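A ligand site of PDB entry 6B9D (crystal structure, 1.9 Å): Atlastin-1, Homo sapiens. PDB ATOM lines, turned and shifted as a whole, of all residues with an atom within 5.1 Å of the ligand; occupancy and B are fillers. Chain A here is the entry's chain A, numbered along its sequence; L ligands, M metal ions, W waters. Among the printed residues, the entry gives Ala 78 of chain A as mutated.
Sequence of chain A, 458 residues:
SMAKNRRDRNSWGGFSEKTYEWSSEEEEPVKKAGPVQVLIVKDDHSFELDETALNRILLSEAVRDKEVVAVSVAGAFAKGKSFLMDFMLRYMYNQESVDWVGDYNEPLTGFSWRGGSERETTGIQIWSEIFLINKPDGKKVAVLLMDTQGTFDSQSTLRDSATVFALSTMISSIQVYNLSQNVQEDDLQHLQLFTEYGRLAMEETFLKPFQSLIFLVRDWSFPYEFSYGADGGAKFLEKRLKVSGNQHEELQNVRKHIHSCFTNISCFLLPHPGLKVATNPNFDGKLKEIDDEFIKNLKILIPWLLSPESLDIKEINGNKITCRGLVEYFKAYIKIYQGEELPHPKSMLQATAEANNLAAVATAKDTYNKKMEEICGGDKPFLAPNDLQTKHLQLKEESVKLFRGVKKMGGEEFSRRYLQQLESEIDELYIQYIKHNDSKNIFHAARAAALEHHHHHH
The side-chain amide oxygen (OE1) of Gln 149 lies within hydrogen-bond range of the side-chain amino group (NZ) of Lys 81 (2.5 Å). The backbone carbonyl oxygen (O) of Ala 76 sits at hydrogen-bond distance from the side-chain amino group (NZ) of Lys 81 (3.1 Å). The side-chain amide oxygen (OD1) of Asn 280 is in hydrogen-bond range of the side-chain hydroxyl (OG1) of Thr 279, 3.1 Å away. The guanidinium group (NH2) of Arg 218 lies within hydrogen-bond range of the backbone carbonyl oxygen (O) of Gly 80 (3.1 Å). The guanidinium group of Arg 218 lies within hydrogen-bond range of the side-chain amide oxygen of Asn 178 (2.9 Å). The side-chain hydroxyl of Ser 82 is in hydrogen-bond range of the side-chain carboxylate of Asp 147 (3.0 Å). The side-chain amide nitrogen of Asn 178 lies within hydrogen-bond range of the backbone carbonyl oxygen of Lys 79 (2.9 Å).
Water W3 lies within hydrogen-bond range of the backbone carbonyl oxygen (O) of Pro 271 (2.6 Å), an oxygen (O11) of the ligand (2.6 Å), the backbone NH (N) of Asp 219 (3.0 Å) and the guanidinium group (NE) of Arg 218 (3.4 Å). Water W1 lies within hydrogen-bond range of an oxygen (O8) of the ligand and the backbone carbonyl oxygen of Ala 78. Water W2 lies within hydrogen-bond range of the backbone carbonyl oxygen of Pro 281 (2.8 Å), the backbone NH of Phe 283 (3.0 Å) and an oxygen (O10) of the ligand (3.1 Å). Water W4 bridges O of Lys 79 (3.2 Å) and N3 of the ligand (3.2 Å).
O of Ala 76 touches O2 of the ligand, 3.9 Å away. C of Phe 77 touches O1 of the ligand, at 3.8 Å. Pro 273 touches the ligand (CD to N3, 3.2 Å). Ala 278 touches the ligand (CB to N4, 3.9 Å). CA of Pro 281 touches O9 of the ligand, at 3.4 Å. CB of Phe 283 touches O10 of the ligand, at 3.998 Å. Phe 294 touches the ligand.
The backbone NH (N) of Lys 81 is in hydrogen-bond range of an oxygen (O2) of the ligand. O2 of the ligand is in salt-bridge range of NZ of Lys 81, 2.6 Å away. The side-chain carboxylate (OD1) of Asp 219 lies within hydrogen-bond range of a nitrogen (N3) of the ligand. The backbone carbonyl oxygen (O) of Asn 280 is in hydrogen-bond range of an oxygen (O9) of the ligand (2.7 Å). The backbone NH (N) of Ala 78 sits at hydrogen-bond distance from an oxygen (O1) of the ligand, at 2.7 Å. NH2 of Arg 218 lies within hydrogen-bond range of N2 of the ligand, 2.8 Å away. O of Val 277 sits at hydrogen-bond distance from O10 of the ligand (2.8 Å). The side-chain amide nitrogen (NE2) of Gln 149 lies within hydrogen-bond range of an oxygen (O1) of the ligand (2.8 Å). An oxygen (O4) of the ligand sits at hydrogen-bond distance from the backbone NH (N) of Gly 80 (2.9 Å). An oxygen (O3) of the ligand lies within hydrogen-bond range of the backbone NH (N) of Ser 82, 2.9 Å away. OG of Ser 82 lies within hydrogen-bond range of O3 of the ligand (2.9 Å). N of Phe 83 is in hydrogen-bond range of O6 of the ligand, at 3.0 Å. N of Lys 79 is in hydrogen-bond range of O2 of the ligand (3.1 Å).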
ATOM      1  N   ALA A  76      30.138 -11.566  -7.088  1.00  0.00           N
ATOM      2  CA  ALA A  76      30.387 -10.156  -7.368  1.00  0.00           C
ATOM      3  C   ALA A  76      29.145  -9.419  -7.845  1.00  0.00           C
ATOM      4  O   ALA A  76      28.224 -10.022  -8.415  1.00  0.00           O
ATOM      5  CB  ALA A  76      31.507 -10.031  -8.398  1.00  0.00           C
ATOM      6  N   PHE A  77      29.133  -8.099  -7.650  1.00  0.00           N
ATOM      7  CA  PHE A  77      27.987  -7.275  -8.004  1.00  0.00           C
ATOM      8  C   PHE A  77      27.726  -7.270  -9.507  1.00  0.00           C
ATOM      9  O   PHE A  77      28.653  -7.326 -10.315  1.00  0.00           O
ATOM     10  CB  PHE A  77      28.199  -5.839  -7.509  1.00  0.00           C
ATOM     11  N   ALA A  78      26.449  -7.209  -9.868  1.00  0.00           N
ATOM     12  CA  ALA A  78      26.015  -6.947 -11.243  1.00  0.00           C
ATOM     13  C   ALA A  78      26.443  -8.060 -12.192  1.00  0.00           C
ATOM     14  O   ALA A  78      26.719  -7.805 -13.367  1.00  0.00           O
ATOM     15  CB  ALA A  78      26.510  -5.587 -11.741  1.00  0.00           C
ATOM     16  N   LYS A  79      26.457  -9.301 -11.702  1.00  0.00           N
ATOM     17  CA  LYS A  79      26.797 -10.449 -12.532  1.00  0.00           C
ATOM     18  C   LYS A  79      25.598 -11.391 -12.745  1.00  0.00           C
ATOM     19  O   LYS A  79      25.782 -12.551 -13.109  1.00  0.00           O
ATOM     20  CB  LYS A  79      27.987 -11.210 -11.946  1.00  0.00           C
ATOM     21  CG  LYS A  79      29.311 -10.421 -11.902  1.00  0.00           C
ATOM     22  CD  LYS A  79      29.772 -10.009 -13.317  1.00  0.00           C
ATOM     23  CE  LYS A  79      31.082  -9.243 -13.269  1.00  0.00           C
ATOM     24  NZ  LYS A  79      31.332  -8.483 -14.547  1.00  0.00           N
ATOM     25  N   GLY A  80      24.372 -10.899 -12.530  1.00  0.00           N
ATOM     26  CA  GLY A  80      23.170 -11.629 -12.881  1.00  0.00           C
ATOM     27  C   GLY A  80      22.557 -12.498 -11.808  1.00  0.00           C
ATOM     28  O   GLY A  80      21.760 -13.392 -12.137  1.00  0.00           O
ATOM     29  N   LYS A  81      22.882 -12.271 -10.533  1.00  0.00           N
ATOM     30  CA  LYS A  81      22.388 -13.120  -9.462  1.00  0.00           C
ATOM     31  C   LYS A  81      20.885 -12.956  -9.262  1.00  0.00           C
ATOM     32  O   LYS A  81      20.161 -13.951  -9.192  1.00  0.00           O
ATOM     33  CB  LYS A  81      23.142 -12.813  -8.164  1.00  0.00           C
ATOM     34  CG  LYS A  81      24.657 -13.029  -8.279  1.00  0.00           C
ATOM     35  CD  LYS A  81      25.337 -12.989  -6.909  1.00  0.00           C
ATOM     36  CE  LYS A  81      25.114 -11.651  -6.216  1.00  0.00           C
ATOM     37  NZ  LYS A  81      25.471 -10.462  -7.040  1.00  0.00           N
ATOM     38  N   SER A  82      20.405 -11.718  -9.144  1.00  0.00           N
ATOM     39  CA  SER A  82      18.972 -11.482  -8.964  1.00  0.00           C
ATOM     40  C   SER A  82      18.183 -11.970 -10.172  1.00  0.00           C
ATOM     41  O   SER A  82      17.064 -12.493 -10.032  1.00  0.00           O
ATOM     42  CB  SER A  82      18.705 -10.002  -8.721  1.00  0.00           C
ATOM     43  OG  SER A  82      19.479  -9.531  -7.625  1.00  0.00           O
ATOM     44  N   PHE A  83      18.733 -11.774 -11.368  1.00  0.00           N
ATOM     45  CA  PHE A  83      18.095 -12.280 -12.591  1.00  0.00           C
ATOM     46  C   PHE A  83      17.930 -13.791 -12.519  1.00  0.00           C
ATOM     47  O   PHE A  83      16.851 -14.324 -12.790  1.00  0.00           O
ATOM     48  CB  PHE A  83      18.963 -11.876 -13.796  1.00  0.00           C
ATOM     49  CG  PHE A  83      18.373 -12.197 -15.138  1.00  0.00           C
ATOM     50  CD1 PHE A  83      17.480 -11.341 -15.741  1.00  0.00           C
ATOM     51  CD2 PHE A  83      18.784 -13.310 -15.850  1.00  0.00           C
ATOM     52  CE1 PHE A  83      16.943 -11.613 -16.996  1.00  0.00           C
ATOM     53  CE2 PHE A  83      18.274 -13.583 -17.114  1.00  0.00           C
ATOM     54  CZ  PHE A  83      17.355 -12.730 -17.684  1.00  0.00           C
ATOM     55  N   SER A 112      15.318  -7.589  -6.774  1.00  0.00           N
ATOM     56  CA  SER A 112      15.646  -6.488  -7.676  1.00  0.00           C
ATOM     57  C   SER A 112      17.153  -6.291  -7.787  1.00  0.00           C
ATOM     58  O   SER A 112      17.739  -6.439  -8.867  1.00  0.00           O
ATOM     59  CB  SER A 112      14.966  -5.197  -7.203  1.00  0.00           C
ATOM     60  OG  SER A 112      13.571  -5.383  -7.026  1.00  0.00           O
ATOM     61  N   ASP A 147      19.715 -14.132  -1.405  1.00  0.00           N
ATOM     62  CA  ASP A 147      20.512 -13.415  -2.386  1.00  0.00           C
ATOM     63  C   ASP A 147      21.638 -12.735  -1.615  1.00  0.00           C
ATOM     64  O   ASP A 147      21.387 -11.835  -0.805  1.00  0.00           O
ATOM     65  CB  ASP A 147      19.665 -12.406  -3.152  1.00  0.00           C
ATOM     66  CG  ASP A 147      20.391 -11.841  -4.353  1.00  0.00           C
ATOM     67  OD1 ASP A 147      21.576 -12.173  -4.549  1.00  0.00           O
ATOM     68  OD2 ASP A 147      19.788 -11.047  -5.086  1.00  0.00           O
ATOM     69  N   GLN A 149      24.739 -10.454  -1.734  1.00  0.00           N
ATOM     70  CA  GLN A 149      25.279  -9.435  -2.619  1.00  0.00           C
ATOM     71  C   GLN A 149      26.583  -8.880  -2.058  1.00  0.00           C
ATOM     72  O   GLN A 149      26.652  -8.478  -0.897  1.00  0.00           O
ATOM     73  CB  GLN A 149      24.246  -8.312  -2.819  1.00  0.00           C
ATOM     74  CG  GLN A 149      24.685  -7.194  -3.770  1.00  0.00           C
ATOM     75  CD  GLN A 149      24.880  -7.674  -5.205  1.00  0.00           C
ATOM     76  OE1 GLN A 149      25.772  -8.463  -5.495  1.00  0.00           O
ATOM     77  NE2 GLN A 149      24.014  -7.201  -6.110  1.00  0.00           N
ATOM     78  N   ASN A 178      28.363 -17.589  -8.108  1.00  0.00           N
ATOM     79  CA  ASN A 178      28.078 -17.032  -9.425  1.00  0.00           C
ATOM     80  C   ASN A 178      29.320 -16.310  -9.928  1.00  0.00           C
ATOM     81  O   ASN A 178      29.730 -15.308  -9.338  1.00  0.00           O
ATOM     82  CB  ASN A 178      26.893 -16.072  -9.353  1.00  0.00           C
ATOM     83  CG  ASN A 178      26.401 -15.665 -10.716  1.00  0.00           C
ATOM     84  OD1 ASN A 178      25.900 -16.497 -11.459  1.00  0.00           O
ATOM     85  ND2 ASN A 178      26.455 -14.382 -11.008  1.00  0.00           N
ATOM     86  N   ARG A 218      28.898 -17.895 -15.648  1.00  0.00           N
ATOM     87  CA  ARG A 218      28.091 -17.149 -16.607  1.00  0.00           C
ATOM     88  C   ARG A 218      28.906 -16.792 -17.832  1.00  0.00           C
ATOM     89  O   ARG A 218      30.128 -16.644 -17.763  1.00  0.00           O
ATOM     90  CB  ARG A 218      27.526 -15.882 -15.966  1.00  0.00           C
ATOM     91  CG  ARG A 218      26.793 -16.171 -14.638  1.00  0.00           C
ATOM     92  CD  ARG A 218      25.494 -16.950 -14.830  1.00  0.00           C
ATOM     93  NE  ARG A 218      24.455 -16.019 -15.254  1.00  0.00           N
ATOM     94  CZ  ARG A 218      23.580 -15.467 -14.423  1.00  0.00           C
ATOM     95  NH1 ARG A 218      23.614 -15.769 -13.122  1.00  0.00           N
ATOM     96  NH2 ARG A 218      22.680 -14.605 -14.871  1.00  0.00           N
ATOM     97  N   ASP A 219      28.216 -16.635 -18.960  1.00  0.00           N
ATOM     98  CA  ASP A 219      28.831 -16.180 -20.212  1.00  0.00           C
ATOM     99  C   ASP A 219      30.019 -17.071 -20.612  1.00  0.00           C
ATOM    100  O   ASP A 219      31.102 -16.580 -20.923  1.00  0.00           O
ATOM    101  CB  ASP A 219      29.280 -14.720 -20.125  1.00  0.00           C
ATOM    102  CG  ASP A 219      28.147 -13.749 -19.857  1.00  0.00           C
ATOM    103  OD1 ASP A 219      26.972 -14.190 -19.867  1.00  0.00           O
ATOM    104  OD2 ASP A 219      28.436 -12.552 -19.621  1.00  0.00           O
ATOM    105  N   PRO A 271      25.444 -20.321 -21.095  1.00  0.00           N
ATOM    106  CA  PRO A 271      25.710 -19.381 -22.189  1.00  0.00           C
ATOM    107  C   PRO A 271      25.396 -17.942 -21.816  1.00  0.00           C
ATOM    108  O   PRO A 271      24.656 -17.643 -20.874  1.00  0.00           O
ATOM    109  CB  PRO A 271      24.794 -19.857 -23.329  1.00  0.00           C
ATOM    110  CG  PRO A 271      23.893 -20.839 -22.767  1.00  0.00           C
ATOM    111  CD  PRO A 271      24.438 -21.325 -21.437  1.00  0.00           C
ATOM    112  N   HIS A 272      25.995 -17.058 -22.603  1.00  0.00           N
ATOM    113  CA  HIS A 272      25.626 -15.646 -22.632  1.00  0.00           C
ATOM    114  C   HIS A 272      24.135 -15.515 -22.992  1.00  0.00           C
ATOM    115  O   HIS A 272      23.626 -16.275 -23.833  1.00  0.00           O
ATOM    116  CB  HIS A 272      26.542 -14.945 -23.636  1.00  0.00           C
ATOM    117  CG  HIS A 272      26.342 -13.468 -23.769  1.00  0.00           C
ATOM    118  ND1 HIS A 272      27.227 -12.544 -23.249  1.00  0.00           N
ATOM    119  CD2 HIS A 272      25.403 -12.760 -24.428  1.00  0.00           C
ATOM    120  CE1 HIS A 272      26.814 -11.333 -23.545  1.00  0.00           C
ATOM    121  NE2 HIS A 272      25.699 -11.434 -24.251  1.00  0.00           N
ATOM    122  N   PRO A 273      23.398 -14.609 -22.341  1.00  0.00           N
ATOM    123  CA  PRO A 273      21.945 -14.540 -22.538  1.00  0.00           C
ATOM    124  C   PRO A 273      21.494 -13.665 -23.692  1.00  0.00           C
ATOM    125  O   PRO A 273      20.292 -13.516 -23.904  1.00  0.00           O
ATOM    126  CB  PRO A 273      21.473 -13.937 -21.207  1.00  0.00           C
ATOM    127  CG  PRO A 273      22.584 -12.944 -20.907  1.00  0.00           C
ATOM    128  CD  PRO A 273      23.853 -13.659 -21.304  1.00  0.00           C
ATOM    129  N   VAL A 277      19.519  -8.835 -22.742  1.00  0.00           N
ATOM    130  CA  VAL A 277      19.749  -9.058 -21.309  1.00  0.00           C
ATOM    131  C   VAL A 277      21.036  -8.369 -20.860  1.00  0.00           C
ATOM    132  O   VAL A 277      21.062  -7.718 -19.804  1.00  0.00           O
ATOM    133  CB  VAL A 277      19.788 -10.561 -21.008  1.00  0.00           C
ATOM    134  CG1 VAL A 277      20.119 -10.797 -19.542  1.00  0.00           C
ATOM    135  CG2 VAL A 277      18.460 -11.213 -21.387  1.00  0.00           C
ATOM    136  N   ALA A 278      22.093  -8.484 -21.652  1.00  0.00           N
ATOM    137  CA  ALA A 278      23.419  -8.046 -21.218  1.00  0.00           C
ATOM    138  C   ALA A 278      23.519  -6.529 -21.042  1.00  0.00           C
ATOM    139  O   ALA A 278      24.443  -6.068 -20.362  1.00  0.00           O
ATOM    140  CB  ALA A 278      24.490  -8.516 -22.204  1.00  0.00           C
ATOM    141  N   THR A 279      22.618  -5.750 -21.639  1.00  0.00           N
ATOM    142  CA  THR A 279      22.815  -4.306 -21.699  1.00  0.00           C
ATOM    143  C   THR A 279      21.814  -3.475 -20.895  1.00  0.00           C
ATOM    144  O   THR A 279      22.091  -2.293 -20.650  1.00  0.00           O
ATOM    145  CB  THR A 279      22.787  -3.833 -23.155  1.00  0.00           C
ATOM    146  OG1 THR A 279      21.528  -4.172 -23.754  1.00  0.00           O
ATOM    147  CG2 THR A 279      23.936  -4.483 -23.935  1.00  0.00           C
ATOM    148  N   ASN A 280      20.669  -4.023 -20.498  1.00  0.00           N
ATOM    149  CA  ASN A 280      19.672  -3.226 -19.788  1.00  0.00           C
ATOM    150  C   ASN A 280      19.560  -3.685 -18.352  1.00  0.00           C
ATOM    151  O   ASN A 280      19.265  -4.864 -18.097  1.00  0.00           O
ATOM    152  CB  ASN A 280      18.323  -3.282 -20.506  1.00  0.00           C
ATOM    153  CG  ASN A 280      18.325  -2.475 -21.790  1.00  0.00           C
ATOM    154  OD1 ASN A 280      18.846  -2.931 -22.816  1.00  0.00           O
ATOM    155  ND2 ASN A 280      17.786  -1.254 -21.732  1.00  0.00           N
ATOM    156  N   PRO A 281      19.752  -2.781 -17.380  1.00  0.00           N
ATOM    157  CA  PRO A 281      19.704  -3.197 -15.958  1.00  0.00           C
ATOM    158  C   PRO A 281      18.363  -3.771 -15.520  1.00  0.00           C
ATOM    159  O   PRO A 281      18.313  -4.856 -14.924  1.00  0.00           O
ATOM    160  CB  PRO A 281      20.035  -1.897 -15.209  1.00  0.00           C
ATOM    161  CG  PRO A 281      20.677  -1.002 -16.224  1.00  0.00           C
ATOM    162  CD  PRO A 281      20.033  -1.350 -17.524  1.00  0.00           C
ATOM    163  N   PHE A 283      15.858  -5.268 -17.092  1.00  0.00           N
ATOM    164  CA  PHE A 283      15.454  -5.908 -18.337  1.00  0.00           C
ATOM    165  C   PHE A 283      14.020  -6.403 -18.206  1.00  0.00           C
ATOM    166  O   PHE A 283      13.748  -7.474 -17.670  1.00  0.00           O
ATOM    167  CB  PHE A 283      16.396  -7.058 -18.669  1.00  0.00           C
ATOM    168  CG  PHE A 283      15.937  -7.891 -19.816  1.00  0.00           C
ATOM    169  CD1 PHE A 283      15.981  -7.392 -21.106  1.00  0.00           C
ATOM    170  CD2 PHE A 283      15.426  -9.158 -19.620  1.00  0.00           C
ATOM    171  CE1 PHE A 283      15.547  -8.158 -22.163  1.00  0.00           C
ATOM    172  CE2 PHE A 283      14.990  -9.921 -20.663  1.00  0.00           C
ATOM    173  CZ  PHE A 283      15.044  -9.418 -21.944  1.00  0.00           C
ATOM    174  N   PHE A 294      20.554 -19.904 -23.964  1.00  0.00           N
ATOM    175  CA  PHE A 294      20.485 -19.575 -22.540  1.00  0.00           C
ATOM    176  C   PHE A 294      19.248 -20.194 -21.901  1.00  0.00           C
ATOM    177  O   PHE A 294      19.327 -20.857 -20.853  1.00  0.00           O
ATOM    178  CB  PHE A 294      20.484 -18.063 -22.355  1.00  0.00           C
ATOM    179  CG  PHE A 294      20.478 -17.602 -20.911  1.00  0.00           C
ATOM    180  CD1 PHE A 294      21.671 -17.463 -20.199  1.00  0.00           C
ATOM    181  CD2 PHE A 294      19.290 -17.292 -20.257  1.00  0.00           C
ATOM    182  CE1 PHE A 294      21.677 -17.021 -18.875  1.00  0.00           C
ATOM    183  CE2 PHE A 294      19.285 -16.853 -18.942  1.00  0.00           C
ATOM    184  CZ  PHE A 294      20.495 -16.718 -18.247  1.00  0.00           C
HETATM  185  P1  LIG L   1      23.426  -8.983  -9.520  1.00  0.00           P
HETATM  186  O1  LIG L   1      23.984  -7.747  -8.891  1.00  0.00           O
HETATM  187  O2  LIG L   1      24.480 -10.051  -9.459  1.00  0.00           O
HETATM  188  O3  LIG L   1      22.168  -9.415  -8.782  1.00  0.00           O
HETATM  189  O4  LIG L   1      23.113  -8.706 -11.069  1.00  0.00           O
HETATM  190  P2  LIG L   1      21.669  -8.392 -11.706  1.00  0.00           P
HETATM  191  O5  LIG L   1      21.057  -7.111 -11.207  1.00  0.00           O
HETATM  192  O6  LIG L   1      20.783  -9.601 -11.607  1.00  0.00           O
HETATM  193  O7  LIG L   1      22.076  -8.220 -13.257  1.00  0.00           O
HETATM  194  C1  LIG L   1      22.807  -7.086 -13.721  1.00  0.00           C
HETATM  195  C2  LIG L   1      22.775  -7.057 -15.257  1.00  0.00           C
HETATM  196  O8  LIG L   1      23.226  -8.306 -15.793  1.00  0.00           O
HETATM  197  C3  LIG L   1      21.353  -6.902 -15.767  1.00  0.00           C
HETATM  198  O9  LIG L   1      21.391  -6.005 -16.889  1.00  0.00           O
HETATM  199  C4  LIG L   1      20.967  -8.274 -16.250  1.00  0.00           C
HETATM  200  O10 LIG L   1      19.959  -8.218 -17.274  1.00  0.00           O
HETATM  201  C5  LIG L   1      22.299  -8.781 -16.770  1.00  0.00           C
HETATM  202  N1  LIG L   1      22.437 -10.252 -16.818  1.00  0.00           N
HETATM  203  C6  LIG L   1      21.671 -11.211 -16.233  1.00  0.00           C
HETATM  204  N2  LIG L   1      22.159 -12.455 -16.506  1.00  0.00           N
HETATM  205  C7  LIG L   1      23.277 -12.286 -17.279  1.00  0.00           C
HETATM  206  C8  LIG L   1      24.304 -13.154 -17.916  1.00  0.00           C
HETATM  207  O11 LIG L   1      24.228 -14.416 -17.823  1.00  0.00           O
HETATM  208  N3  LIG L   1      25.288 -12.556 -18.641  1.00  0.00           N
HETATM  209  C9  LIG L   1      25.369 -11.221 -18.770  1.00  0.00           C
HETATM  210  N4  LIG L   1      26.360 -10.651 -19.492  1.00  0.00           N
HETATM  211  N5  LIG L   1      24.485 -10.373 -18.194  1.00  0.00           N
HETATM  212  C10 LIG L   1      23.447 -10.846 -17.464  1.00  0.00           C
HETATM  213 MG    MG M   1      22.246  -9.551  -5.729  1.00  0.00          MG
HETATM  214  O   HOH W   1      26.048  -8.978 -16.064  1.00  0.00           O
HETATM  215  O   HOH W   2      17.482  -7.395 -15.663  1.00  0.00           O
HETATM  216  O   HOH W   3      25.221 -16.779 -18.463  1.00  0.00           O
HETATM  217  O   HOH W   4      26.912 -11.751 -15.985  1.00  0.00           O
